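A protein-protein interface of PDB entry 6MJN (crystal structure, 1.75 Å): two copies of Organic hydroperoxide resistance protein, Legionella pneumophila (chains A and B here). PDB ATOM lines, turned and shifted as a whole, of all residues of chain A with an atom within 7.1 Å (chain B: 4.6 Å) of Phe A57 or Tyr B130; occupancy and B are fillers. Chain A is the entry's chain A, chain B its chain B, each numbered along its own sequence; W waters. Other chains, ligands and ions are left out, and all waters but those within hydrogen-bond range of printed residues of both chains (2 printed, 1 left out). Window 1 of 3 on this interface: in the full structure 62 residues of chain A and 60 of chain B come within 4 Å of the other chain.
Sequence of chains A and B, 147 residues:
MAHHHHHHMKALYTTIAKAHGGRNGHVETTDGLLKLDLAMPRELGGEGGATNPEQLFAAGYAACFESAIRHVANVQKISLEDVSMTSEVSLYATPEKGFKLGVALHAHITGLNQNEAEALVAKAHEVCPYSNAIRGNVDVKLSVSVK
The backbone NH (N) of Phe B57 sits at hydrogen-bond distance from the side-chain hydroxyl (OH) of Tyr A130 (3.4 Å).
The side-chain hydroxyl of Tyr B130 sits at hydrogen-bond distance from the backbone carbonyl oxygen of Pro A53, at 2.7 Å.
The side-chain sulfur (SG) of Cys B64 sits at hydrogen-bond distance from the side-chain sulfur (SG) of Cys B128.
SG of Cys B128 lies close to N of Tyr B130, 3.6 Å away.
Pro A53 touches Gly B60.
Pro A53 touches Cys B64.
CD1 of Leu A56 touches N of Gly B60, 3.7 Å away.
Tyr B130 touches Phe A57.
O of Phe A99 touches CG of Pro B129, at 3.5 Å.
Ala B133 touches Ala A133 (O to O, 3.5 Å).
Ala A133 touches Ile B134.
Ala B133 touches Ile A134.
CG2 of Val A138 touches CB of Ala B133, at 3.6 Å.
Printed residues of chain B within 4 Å of Phe A57: Tyr B130 (3.4 Å).
Gly A60 touches none of the printed residues of chain B.
Printed residues of chain B within 4 Å of Tyr A130: Phe B57 (3.4 Å).
Printed residues of chain A within 4 Å of Gly B60: Pro A53 (3.7 Å) and Leu A56 (3.7 Å).
Tyr B130 touches just these residues of chain A: Pro A53 (2.7 Å) and Phe A57 (3.4 Å).
Ser B131 touches none of the printed residues of chain A.
Of the printed residues of chain A, Ala B133 touches Ala A133, Ile A134 and Val A138.
The nearest printed residue of chain B that does not touch Tyr A130 is Ile B134 (6.4 Å).
Of the 11 printed residues of chain B, 7 touch a printed residue of chain A.
Hydrophobic or aromatic side chains of chain B that line the printed part of chain A: Phe B57, Pro B129, Tyr B130, Ala B133 and Ile B134.
Among the printed residues, 11 pairs touch across the chains.
Phe A57 touches Tyr B130, and with the chains exchanged Tyr A130 touches Phe B57.
Ala B133 touches its own counterpart, Ala A133.
Ala A133 touches Ile B134, and with the chains exchanged Ile A134 touches Ala B133.
Water W1 lies within hydrogen-bond range of the side-chain sulfur of Cys B64 (2.6 Å) and the side-chain carboxylate of Glu A54 (3.4 Å).
Water W2 bridges the backbone carbonyl oxygen (O) of Pro B129 (2.9 Å) and the backbone NH (N) of Leu A101 (3.0 Å).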
ATOM      1  N   ASN A  52      10.732  27.995  12.702  1.00  0.00           N
ATOM      2  CA  ASN A  52      10.716  28.895  11.554  1.00  0.00           C
ATOM      3  C   ASN A  52       9.577  28.462  10.622  1.00  0.00           C
ATOM      4  O   ASN A  52       8.957  27.403  10.832  1.00  0.00           O
ATOM      5  CB  ASN A  52      12.081  28.882  10.827  1.00  0.00           C
ATOM      6  CG  ASN A  52      12.466  27.490  10.334  1.00  0.00           C
ATOM      7  OD1 ASN A  52      11.770  26.900   9.502  1.00  0.00           O
ATOM      8  ND2 ASN A  52      13.597  26.970  10.828  1.00  0.00           N
ATOM      9  N   PRO A  53       9.251  29.266   9.598  1.00  0.00           N
ATOM     10  CA  PRO A  53       8.088  28.915   8.755  1.00  0.00           C
ATOM     11  C   PRO A  53       8.259  27.641   7.944  1.00  0.00           C
ATOM     12  O   PRO A  53       7.253  27.015   7.597  1.00  0.00           O
ATOM     13  CB  PRO A  53       7.939  30.136   7.840  1.00  0.00           C
ATOM     14  CG  PRO A  53       8.536  31.275   8.646  1.00  0.00           C
ATOM     15  CD  PRO A  53       9.694  30.656   9.366  1.00  0.00           C
ATOM     16  N   GLU A  54       9.493  27.238   7.624  1.00  0.00           N
ATOM     17  CA  GLU A  54       9.671  25.982   6.895  1.00  0.00           C
ATOM     18  C   GLU A  54       9.383  24.777   7.789  1.00  0.00           C
ATOM     19  O   GLU A  54       8.814  23.780   7.325  1.00  0.00           O
ATOM     20  CB  GLU A  54      11.077  25.892   6.308  1.00  0.00           C
ATOM     21  CG  GLU A  54      11.335  26.841   5.124  1.00  0.00           C
ATOM     22  CD  GLU A  54      11.232  28.324   5.516  1.00  0.00           C
ATOM     23  OE1 GLU A  54      11.946  28.746   6.445  1.00  0.00           O
ATOM     24  OE2 GLU A  54      10.409  29.054   4.916  1.00  0.00           O
ATOM     25  N   GLN A  55       9.811  24.823   9.050  1.00  0.00           N
ATOM     26  CA  GLN A  55       9.466  23.753   9.984  1.00  0.00           C
ATOM     27  C   GLN A  55       7.967  23.695  10.249  1.00  0.00           C
ATOM     28  O   GLN A  55       7.400  22.598  10.361  1.00  0.00           O
ATOM     29  CB  GLN A  55      10.219  23.924  11.303  1.00  0.00           C
ATOM     30  CG  GLN A  55      11.719  23.743  11.182  1.00  0.00           C
ATOM     31  CD  GLN A  55      12.369  23.546  12.527  1.00  0.00           C
ATOM     32  OE1 GLN A  55      11.877  24.053  13.541  1.00  0.00           O
ATOM     33  NE2 GLN A  55      13.464  22.776  12.558  1.00  0.00           N
ATOM     34  N   LEU A  56       7.312  24.858  10.385  1.00  0.00           N
ATOM     35  CA  LEU A  56       5.865  24.859  10.597  1.00  0.00           C
ATOM     36  C   LEU A  56       5.160  24.189   9.434  1.00  0.00           C
ATOM     37  O   LEU A  56       4.273  23.349   9.646  1.00  0.00           O
ATOM     38  CB  LEU A  56       5.336  26.287  10.797  1.00  0.00           C
ATOM     39  CG  LEU A  56       5.860  26.875  12.116  1.00  0.00           C
ATOM     40  CD1 LEU A  56       5.484  28.314  12.290  1.00  0.00           C
ATOM     41  CD2 LEU A  56       5.359  26.054  13.312  1.00  0.00           C
ATOM     42  N   PHE A  57       5.567  24.521   8.199  1.00  0.00           N
ATOM     43  CA  PHE A  57       4.971  23.898   7.023  1.00  0.00           C
ATOM     44  C   PHE A  57       5.254  22.402   6.999  1.00  0.00           C
ATOM     45  O   PHE A  57       4.352  21.601   6.741  1.00  0.00           O
ATOM     46  CB  PHE A  57       5.492  24.559   5.743  1.00  0.00           C
ATOM     47  CG  PHE A  57       4.819  24.072   4.490  1.00  0.00           C
ATOM     48  CD1 PHE A  57       3.571  24.576   4.107  1.00  0.00           C
ATOM     49  CD2 PHE A  57       5.443  23.145   3.672  1.00  0.00           C
ATOM     50  CE1 PHE A  57       2.949  24.132   2.954  1.00  0.00           C
ATOM     51  CE2 PHE A  57       4.822  22.701   2.519  1.00  0.00           C
ATOM     52  CZ  PHE A  57       3.581  23.194   2.161  1.00  0.00           C
ATOM     53  N   ALA A  58       6.509  22.014   7.270  1.00  0.00           N
ATOM     54  CA  ALA A  58       6.868  20.594   7.286  1.00  0.00           C
ATOM     55  C   ALA A  58       5.999  19.825   8.264  1.00  0.00           C
ATOM     56  O   ALA A  58       5.470  18.755   7.933  1.00  0.00           O
ATOM     57  CB  ALA A  58       8.336  20.419   7.643  1.00  0.00           C
ATOM     58  N   ALA A  59       5.866  20.341   9.485  1.00  0.00           N
ATOM     59  CA  ALA A  59       5.098  19.635  10.509  1.00  0.00           C
ATOM     60  C   ALA A  59       3.616  19.576  10.138  1.00  0.00           C
ATOM     61  O   ALA A  59       2.960  18.537  10.319  1.00  0.00           O
ATOM     62  CB  ALA A  59       5.280  20.321  11.863  1.00  0.00           C
ATOM     63  N   GLY A  60       3.064  20.685   9.659  1.00  0.00           N
ATOM     64  CA  GLY A  60       1.661  20.679   9.299  1.00  0.00           C
ATOM     65  C   GLY A  60       1.385  19.761   8.120  1.00  0.00           C
ATOM     66  O   GLY A  60       0.347  19.089   8.077  1.00  0.00           O
ATOM     67  N   TYR A  61       2.315  19.708   7.155  1.00  0.00           N
ATOM     68  CA  TYR A  61       2.101  18.844   5.990  1.00  0.00           C
ATOM     69  C   TYR A  61       2.164  17.367   6.387  1.00  0.00           C
ATOM     70  O   TYR A  61       1.331  16.559   5.947  1.00  0.00           O
ATOM     71  CB  TYR A  61       3.131  19.167   4.895  1.00  0.00           C
ATOM     72  CG  TYR A  61       2.737  18.794   3.465  1.00  0.00           C
ATOM     73  CD1 TYR A  61       1.595  18.034   3.184  1.00  0.00           C
ATOM     74  CD2 TYR A  61       3.531  19.213   2.390  1.00  0.00           C
ATOM     75  CE1 TYR A  61       1.229  17.733   1.832  1.00  0.00           C
ATOM     76  CE2 TYR A  61       3.224  18.884   1.108  1.00  0.00           C
ATOM     77  CZ  TYR A  61       2.087  18.166   0.825  1.00  0.00           C
ATOM     78  OH  TYR A  61       1.830  17.884  -0.480  1.00  0.00           O
ATOM     79  N   ALA A  62       3.133  17.001   7.228  1.00  0.00           N
ATOM     80  CA  ALA A  62       3.245  15.601   7.668  1.00  0.00           C
ATOM     81  C   ALA A  62       1.988  15.163   8.407  1.00  0.00           C
ATOM     82  O   ALA A  62       1.478  14.057   8.189  1.00  0.00           O
ATOM     83  CB  ALA A  62       4.472  15.405   8.567  1.00  0.00           C
ATOM     84  N   ALA A  63       1.475  16.020   9.287  1.00  0.00           N
ATOM     85  CA  ALA A  63       0.258  15.677  10.021  1.00  0.00           C
ATOM     86  C   ALA A  63      -0.953  15.660   9.090  1.00  0.00           C
ATOM     87  O   ALA A  63      -1.799  14.762   9.174  1.00  0.00           O
ATOM     88  CB  ALA A  63       0.051  16.674  11.168  1.00  0.00           C
ATOM     89  N   SER A  87       7.822  14.291   6.371  1.00  0.00           N
ATOM     90  CA  SER A  87       7.913  15.298   5.331  1.00  0.00           C
ATOM     91  C   SER A  87       9.297  15.920   5.408  1.00  0.00           C
ATOM     92  O   SER A  87       9.870  16.071   6.485  1.00  0.00           O
ATOM     93  CB  SER A  87       6.844  16.400   5.487  1.00  0.00           C
ATOM     94  OG  SER A  87       7.061  17.091   6.705  1.00  0.00           O
ATOM     95  N   VAL A  89      11.183  19.376   3.949  1.00  0.00           N
ATOM     96  CA  VAL A  89      10.932  20.658   3.300  1.00  0.00           C
ATOM     97  C   VAL A  89      12.263  21.369   3.097  1.00  0.00           C
ATOM     98  O   VAL A  89      13.038  21.511   4.048  1.00  0.00           O
ATOM     99  CB  VAL A  89       9.983  21.535   4.123  1.00  0.00           C
ATOM    100  CG1 VAL A  89       9.913  22.943   3.527  1.00  0.00           C
ATOM    101  CG2 VAL A  89       8.597  20.902   4.143  1.00  0.00           C
ATOM    102  N   PHE A  99      13.018  32.957  -2.734  1.00  0.00           N
ATOM    103  CA  PHE A  99      13.182  31.571  -2.324  1.00  0.00           C
ATOM    104  C   PHE A  99      11.923  30.773  -2.648  1.00  0.00           C
ATOM    105  O   PHE A  99      10.821  31.319  -2.719  1.00  0.00           O
ATOM    106  CB  PHE A  99      13.523  31.481  -0.833  1.00  0.00           C
ATOM    107  CG  PHE A  99      14.872  32.064  -0.488  1.00  0.00           C
ATOM    108  CD1 PHE A  99      15.874  32.131  -1.446  1.00  0.00           C
ATOM    109  CD2 PHE A  99      15.136  32.551   0.782  1.00  0.00           C
ATOM    110  CE1 PHE A  99      17.117  32.671  -1.144  1.00  0.00           C
ATOM    111  CE2 PHE A  99      16.380  33.092   1.094  1.00  0.00           C
ATOM    112  CZ  PHE A  99      17.370  33.153   0.129  1.00  0.00           C
ATOM    113  N   LEU A 101       9.892  26.784  -2.105  1.00  0.00           N
ATOM    114  CA  LEU A 101       9.818  25.523  -1.375  1.00  0.00           C
ATOM    115  C   LEU A 101       9.851  24.312  -2.304  1.00  0.00           C
ATOM    116  O   LEU A 101       9.323  24.338  -3.419  1.00  0.00           O
ATOM    117  CB  LEU A 101       8.540  25.450  -0.521  1.00  0.00           C
ATOM    118  CG  LEU A 101       8.342  26.485   0.590  1.00  0.00           C
ATOM    119  CD1 LEU A 101       6.941  26.346   1.180  1.00  0.00           C
ATOM    120  CD2 LEU A 101       9.390  26.341   1.688  1.00  0.00           C
ATOM    121  N   GLY A 102      10.458  23.227  -1.810  1.00  0.00           N
ATOM    122  CA  GLY A 102      10.300  21.916  -2.412  1.00  0.00           C
ATOM    123  C   GLY A 102      10.053  20.914  -1.297  1.00  0.00           C
ATOM    124  O   GLY A 102      10.440  21.144  -0.156  1.00  0.00           O
ATOM    125  N   VAL A 103       9.367  19.811  -1.624  1.00  0.00           N
ATOM    126  CA  VAL A 103       8.894  18.882  -0.586  1.00  0.00           C
ATOM    127  C   VAL A 103       9.140  17.435  -1.006  1.00  0.00           C
ATOM    128  O   VAL A 103       8.926  17.068  -2.167  1.00  0.00           O
ATOM    129  CB  VAL A 103       7.391  19.085  -0.282  1.00  0.00           C
ATOM    130  CG1 VAL A 103       6.902  18.077   0.755  1.00  0.00           C
ATOM    131  CG2 VAL A 103       7.086  20.537   0.191  1.00  0.00           C
ATOM    132  N   TYR A 130      -3.177  20.656   2.256  1.00  0.00           N
ATOM    133  CA  TYR A 130      -1.838  21.169   1.930  1.00  0.00           C
ATOM    134  C   TYR A 130      -1.460  20.810   0.494  1.00  0.00           C
ATOM    135  O   TYR A 130      -0.882  21.631  -0.228  1.00  0.00           O
ATOM    136  CB  TYR A 130      -0.801  20.595   2.898  1.00  0.00           C
ATOM    137  CG  TYR A 130      -0.602  21.329   4.215  1.00  0.00           C
ATOM    138  CD1 TYR A 130      -1.626  21.428   5.145  1.00  0.00           C
ATOM    139  CD2 TYR A 130       0.625  21.859   4.544  1.00  0.00           C
ATOM    140  CE1 TYR A 130      -1.435  22.098   6.362  1.00  0.00           C
ATOM    141  CE2 TYR A 130       0.835  22.494   5.733  1.00  0.00           C
ATOM    142  CZ  TYR A 130      -0.203  22.635   6.636  1.00  0.00           C
ATOM    143  OH  TYR A 130       0.020  23.268   7.847  1.00  0.00           O
ATOM    144  N   SER A 131      -1.741  19.575   0.070  1.00  0.00           N
ATOM    145  CA  SER A 131      -1.378  19.166  -1.288  1.00  0.00           C
ATOM    146  C   SER A 131      -2.138  19.972  -2.306  1.00  0.00           C
ATOM    147  O   SER A 131      -1.575  20.378  -3.316  1.00  0.00           O
ATOM    148  CB  SER A 131      -1.676  17.689  -1.545  1.00  0.00           C
ATOM    149  OG  SER A 131      -0.816  16.898  -0.721  1.00  0.00           O
ATOM    150  N   ALA A 133      -3.329  22.888  -1.876  1.00  0.00           N
ATOM    151  CA  ALA A 133      -2.880  24.278  -1.842  1.00  0.00           C
ATOM    152  C   ALA A 133      -1.654  24.520  -2.727  1.00  0.00           C
ATOM    153  O   ALA A 133      -1.536  25.575  -3.338  1.00  0.00           O
ATOM    154  CB  ALA A 133      -2.570  24.700  -0.404  1.00  0.00           C
ATOM    155  N   ILE A 134      -0.697  23.593  -2.754  1.00  0.00           N
ATOM    156  CA  ILE A 134       0.574  23.863  -3.408  1.00  0.00           C
ATOM    157  C   ILE A 134       0.635  23.232  -4.789  1.00  0.00           C
ATOM    158  O   ILE A 134       1.681  23.285  -5.442  1.00  0.00           O
ATOM    159  CB  ILE A 134       1.756  23.402  -2.539  1.00  0.00           C
ATOM    160  CG1 ILE A 134       1.755  21.875  -2.408  1.00  0.00           C
ATOM    161  CG2 ILE A 134       1.673  24.092  -1.198  1.00  0.00           C
ATOM    162  CD1 ILE A 134       2.869  21.404  -1.458  1.00  0.00           C
ATOM    163  N   VAL A 138       4.769  23.615  -6.402  1.00  0.00           N
ATOM    164  CA  VAL A 138       5.775  23.040  -5.528  1.00  0.00           C
ATOM    165  C   VAL A 138       5.988  21.620  -5.997  1.00  0.00           C
ATOM    166  O   VAL A 138       5.022  20.861  -6.144  1.00  0.00           O
ATOM    167  CB  VAL A 138       5.351  23.096  -4.050  1.00  0.00           C
ATOM    168  CG1 VAL A 138       6.299  22.261  -3.186  1.00  0.00           C
ATOM    169  CG2 VAL A 138       5.304  24.543  -3.569  1.00  0.00           C
ATOM    170  N   PHE B  57      -0.277  26.194   9.467  1.00  0.00           N
ATOM    171  CA  PHE B  57      -0.181  26.903   8.198  1.00  0.00           C
ATOM    172  C   PHE B  57      -0.411  28.397   8.408  1.00  0.00           C
ATOM    173  O   PHE B  57       0.344  29.227   7.886  1.00  0.00           O
ATOM    174  CB  PHE B  57      -1.203  26.339   7.201  1.00  0.00           C
ATOM    175  CG  PHE B  57      -1.043  26.893   5.815  1.00  0.00           C
ATOM    176  CD1 PHE B  57      -0.131  26.314   4.943  1.00  0.00           C
ATOM    177  CD2 PHE B  57      -1.754  28.010   5.416  1.00  0.00           C
ATOM    178  CE1 PHE B  57       0.048  26.818   3.661  1.00  0.00           C
ATOM    179  CE2 PHE B  57      -1.578  28.535   4.148  1.00  0.00           C
ATOM    180  CZ  PHE B  57      -0.668  27.932   3.266  1.00  0.00           C
ATOM    181  N   GLY B  60       2.850  29.782  10.193  1.00  0.00           N
ATOM    182  CA  GLY B  60       3.943  29.892   9.225  1.00  0.00           C
ATOM    183  C   GLY B  60       3.717  30.990   8.193  1.00  0.00           C
ATOM    184  O   GLY B  60       4.643  31.728   7.849  1.00  0.00           O
ATOM    185  N   TYR B  61       2.489  31.105   7.681  1.00  0.00           N
ATOM    186  CA  TYR B  61       2.198  32.117   6.661  1.00  0.00           C
ATOM    187  C   TYR B  61       2.325  33.534   7.230  1.00  0.00           C
ATOM    188  O   TYR B  61       2.951  34.404   6.613  1.00  0.00           O
ATOM    189  CB  TYR B  61       0.793  31.896   6.086  1.00  0.00           C
ATOM    190  CG  TYR B  61       0.555  32.460   4.704  1.00  0.00           C
ATOM    191  CD1 TYR B  61       1.498  33.264   4.081  1.00  0.00           C
ATOM    192  CD2 TYR B  61      -0.631  32.190   4.020  1.00  0.00           C
ATOM    193  CE1 TYR B  61       1.280  33.762   2.810  1.00  0.00           C
ATOM    194  CE2 TYR B  61      -0.860  32.690   2.759  1.00  0.00           C
ATOM    195  CZ  TYR B  61       0.098  33.474   2.163  1.00  0.00           C
ATOM    196  OH  TYR B  61      -0.130  33.978   0.915  1.00  0.00           O
ATOM    197  N   CYS B  64       6.027  34.201   7.618  1.00  0.00           N
ATOM    198  CA  CYS B  64       6.716  34.292   6.339  1.00  0.00           C
ATOM    199  C   CYS B  64       6.388  35.610   5.653  1.00  0.00           C
ATOM    200  O   CYS B  64       7.271  36.260   5.074  1.00  0.00           O
ATOM    201  CB  CYS B  64       6.325  33.090   5.469  1.00  0.00           C
ATOM    202  SG  CYS B  64       7.243  32.987   3.938  1.00  0.00           S
ATOM    203  N   CYS B 128       7.027  36.271  -0.920  1.00  0.00           N
ATOM    204  CA  CYS B 128       6.850  35.309   0.154  1.00  0.00           C
ATOM    205  C   CYS B 128       6.755  33.889  -0.410  1.00  0.00           C
ATOM    206  O   CYS B 128       5.954  33.645  -1.322  1.00  0.00           O
ATOM    207  CB  CYS B 128       5.574  35.693   0.908  1.00  0.00           C
ATOM    208  SG  CYS B 128       4.987  34.546   2.058  1.00  0.00           S
ATOM    209  N   PRO B 129       7.563  32.937   0.075  1.00  0.00           N
ATOM    210  CA  PRO B 129       7.500  31.571  -0.486  1.00  0.00           C
ATOM    211  C   PRO B 129       6.180  30.863  -0.258  1.00  0.00           C
ATOM    212  O   PRO B 129       5.793  30.027  -1.088  1.00  0.00           O
ATOM    213  CB  PRO B 129       8.650  30.845   0.226  1.00  0.00           C
ATOM    214  CG  PRO B 129       9.638  31.933   0.501  1.00  0.00           C
ATOM    215  CD  PRO B 129       8.800  33.153   0.848  1.00  0.00           C
ATOM    216  N   TYR B 130       5.476  31.139   0.845  1.00  0.00           N
ATOM    217  CA  TYR B 130       4.123  30.597   0.989  1.00  0.00           C
ATOM    218  C   TYR B 130       3.202  31.136  -0.098  1.00  0.00           C
ATOM    219  O   TYR B 130       2.393  30.390  -0.663  1.00  0.00           O
ATOM    220  CB  TYR B 130       3.531  30.952   2.344  1.00  0.00           C
ATOM    221  CG  TYR B 130       3.882  30.058   3.527  1.00  0.00           C
ATOM    222  CD1 TYR B 130       5.203  29.819   3.893  1.00  0.00           C
ATOM    223  CD2 TYR B 130       2.867  29.508   4.304  1.00  0.00           C
ATOM    224  CE1 TYR B 130       5.508  29.030   5.006  1.00  0.00           C
ATOM    225  CE2 TYR B 130       3.151  28.722   5.407  1.00  0.00           C
ATOM    226  CZ  TYR B 130       4.478  28.494   5.753  1.00  0.00           C
ATOM    227  OH  TYR B 130       4.740  27.722   6.854  1.00  0.00           O
ATOM    228  N   SER B 131       3.269  32.448  -0.364  1.00  0.00           N
ATOM    229  CA  SER B 131       2.390  33.019  -1.381  1.00  0.00           C
ATOM    230  C   SER B 131       2.671  32.393  -2.735  1.00  0.00           C
ATOM    231  O   SER B 131       1.736  32.096  -3.498  1.00  0.00           O
ATOM    232  CB  SER B 131       2.561  34.544  -1.448  1.00  0.00           C
ATOM    233  OG  SER B 131       2.029  35.197  -0.303  1.00  0.00           O
ATOM    234  N   ASN B 132       3.959  32.192  -3.061  1.00  0.00           N
ATOM    235  CA  ASN B 132       4.300  31.604  -4.348  1.00  0.00           C
ATOM    236  C   ASN B 132       3.876  30.152  -4.412  1.00  0.00           C
ATOM    237  O   ASN B 132       3.462  29.674  -5.477  1.00  0.00           O
ATOM    238  CB  ASN B 132       5.803  31.762  -4.618  1.00  0.00           C
ATOM    239  CG  ASN B 132       6.164  33.188  -4.955  1.00  0.00           C
ATOM    240  OD1 ASN B 132       5.413  33.874  -5.663  1.00  0.00           O
ATOM    241  ND2 ASN B 132       7.296  33.653  -4.442  1.00  0.00           N
ATOM    242  N   ALA B 133       3.923  29.451  -3.275  1.00  0.00           N
ATOM    243  CA  ALA B 133       3.552  28.042  -3.271  1.00  0.00           C
ATOM    244  C   ALA B 133       2.067  27.833  -3.543  1.00  0.00           C
ATOM    245  O   ALA B 133       1.685  26.776  -4.058  1.00  0.00           O
ATOM    246  CB  ALA B 133       3.915  27.401  -1.924  1.00  0.00           C
ATOM    247  N   ILE B 134       1.215  28.808  -3.225  1.00  0.00           N
ATOM    248  CA  ILE B 134      -0.226  28.604  -3.339  1.00  0.00           C
ATOM    249  C   ILE B 134      -0.848  29.451  -4.443  1.00  0.00           C
ATOM    250  O   ILE B 134      -2.069  29.441  -4.594  1.00  0.00           O
ATOM    251  CB  ILE B 134      -0.928  28.842  -1.996  1.00  0.00           C
ATOM    252  CG1 ILE B 134      -0.875  30.340  -1.609  1.00  0.00           C
ATOM    253  CG2 ILE B 134      -0.283  27.953  -0.928  1.00  0.00           C
ATOM    254  CD1 ILE B 134      -1.491  30.687  -0.208  1.00  0.00           C
HETATM  255  O   HOH W   1       9.503  32.327   4.959  1.00  0.00           O
HETATM  256  O   HOH W   2       7.357  28.317  -2.754  1.00  0.00           O
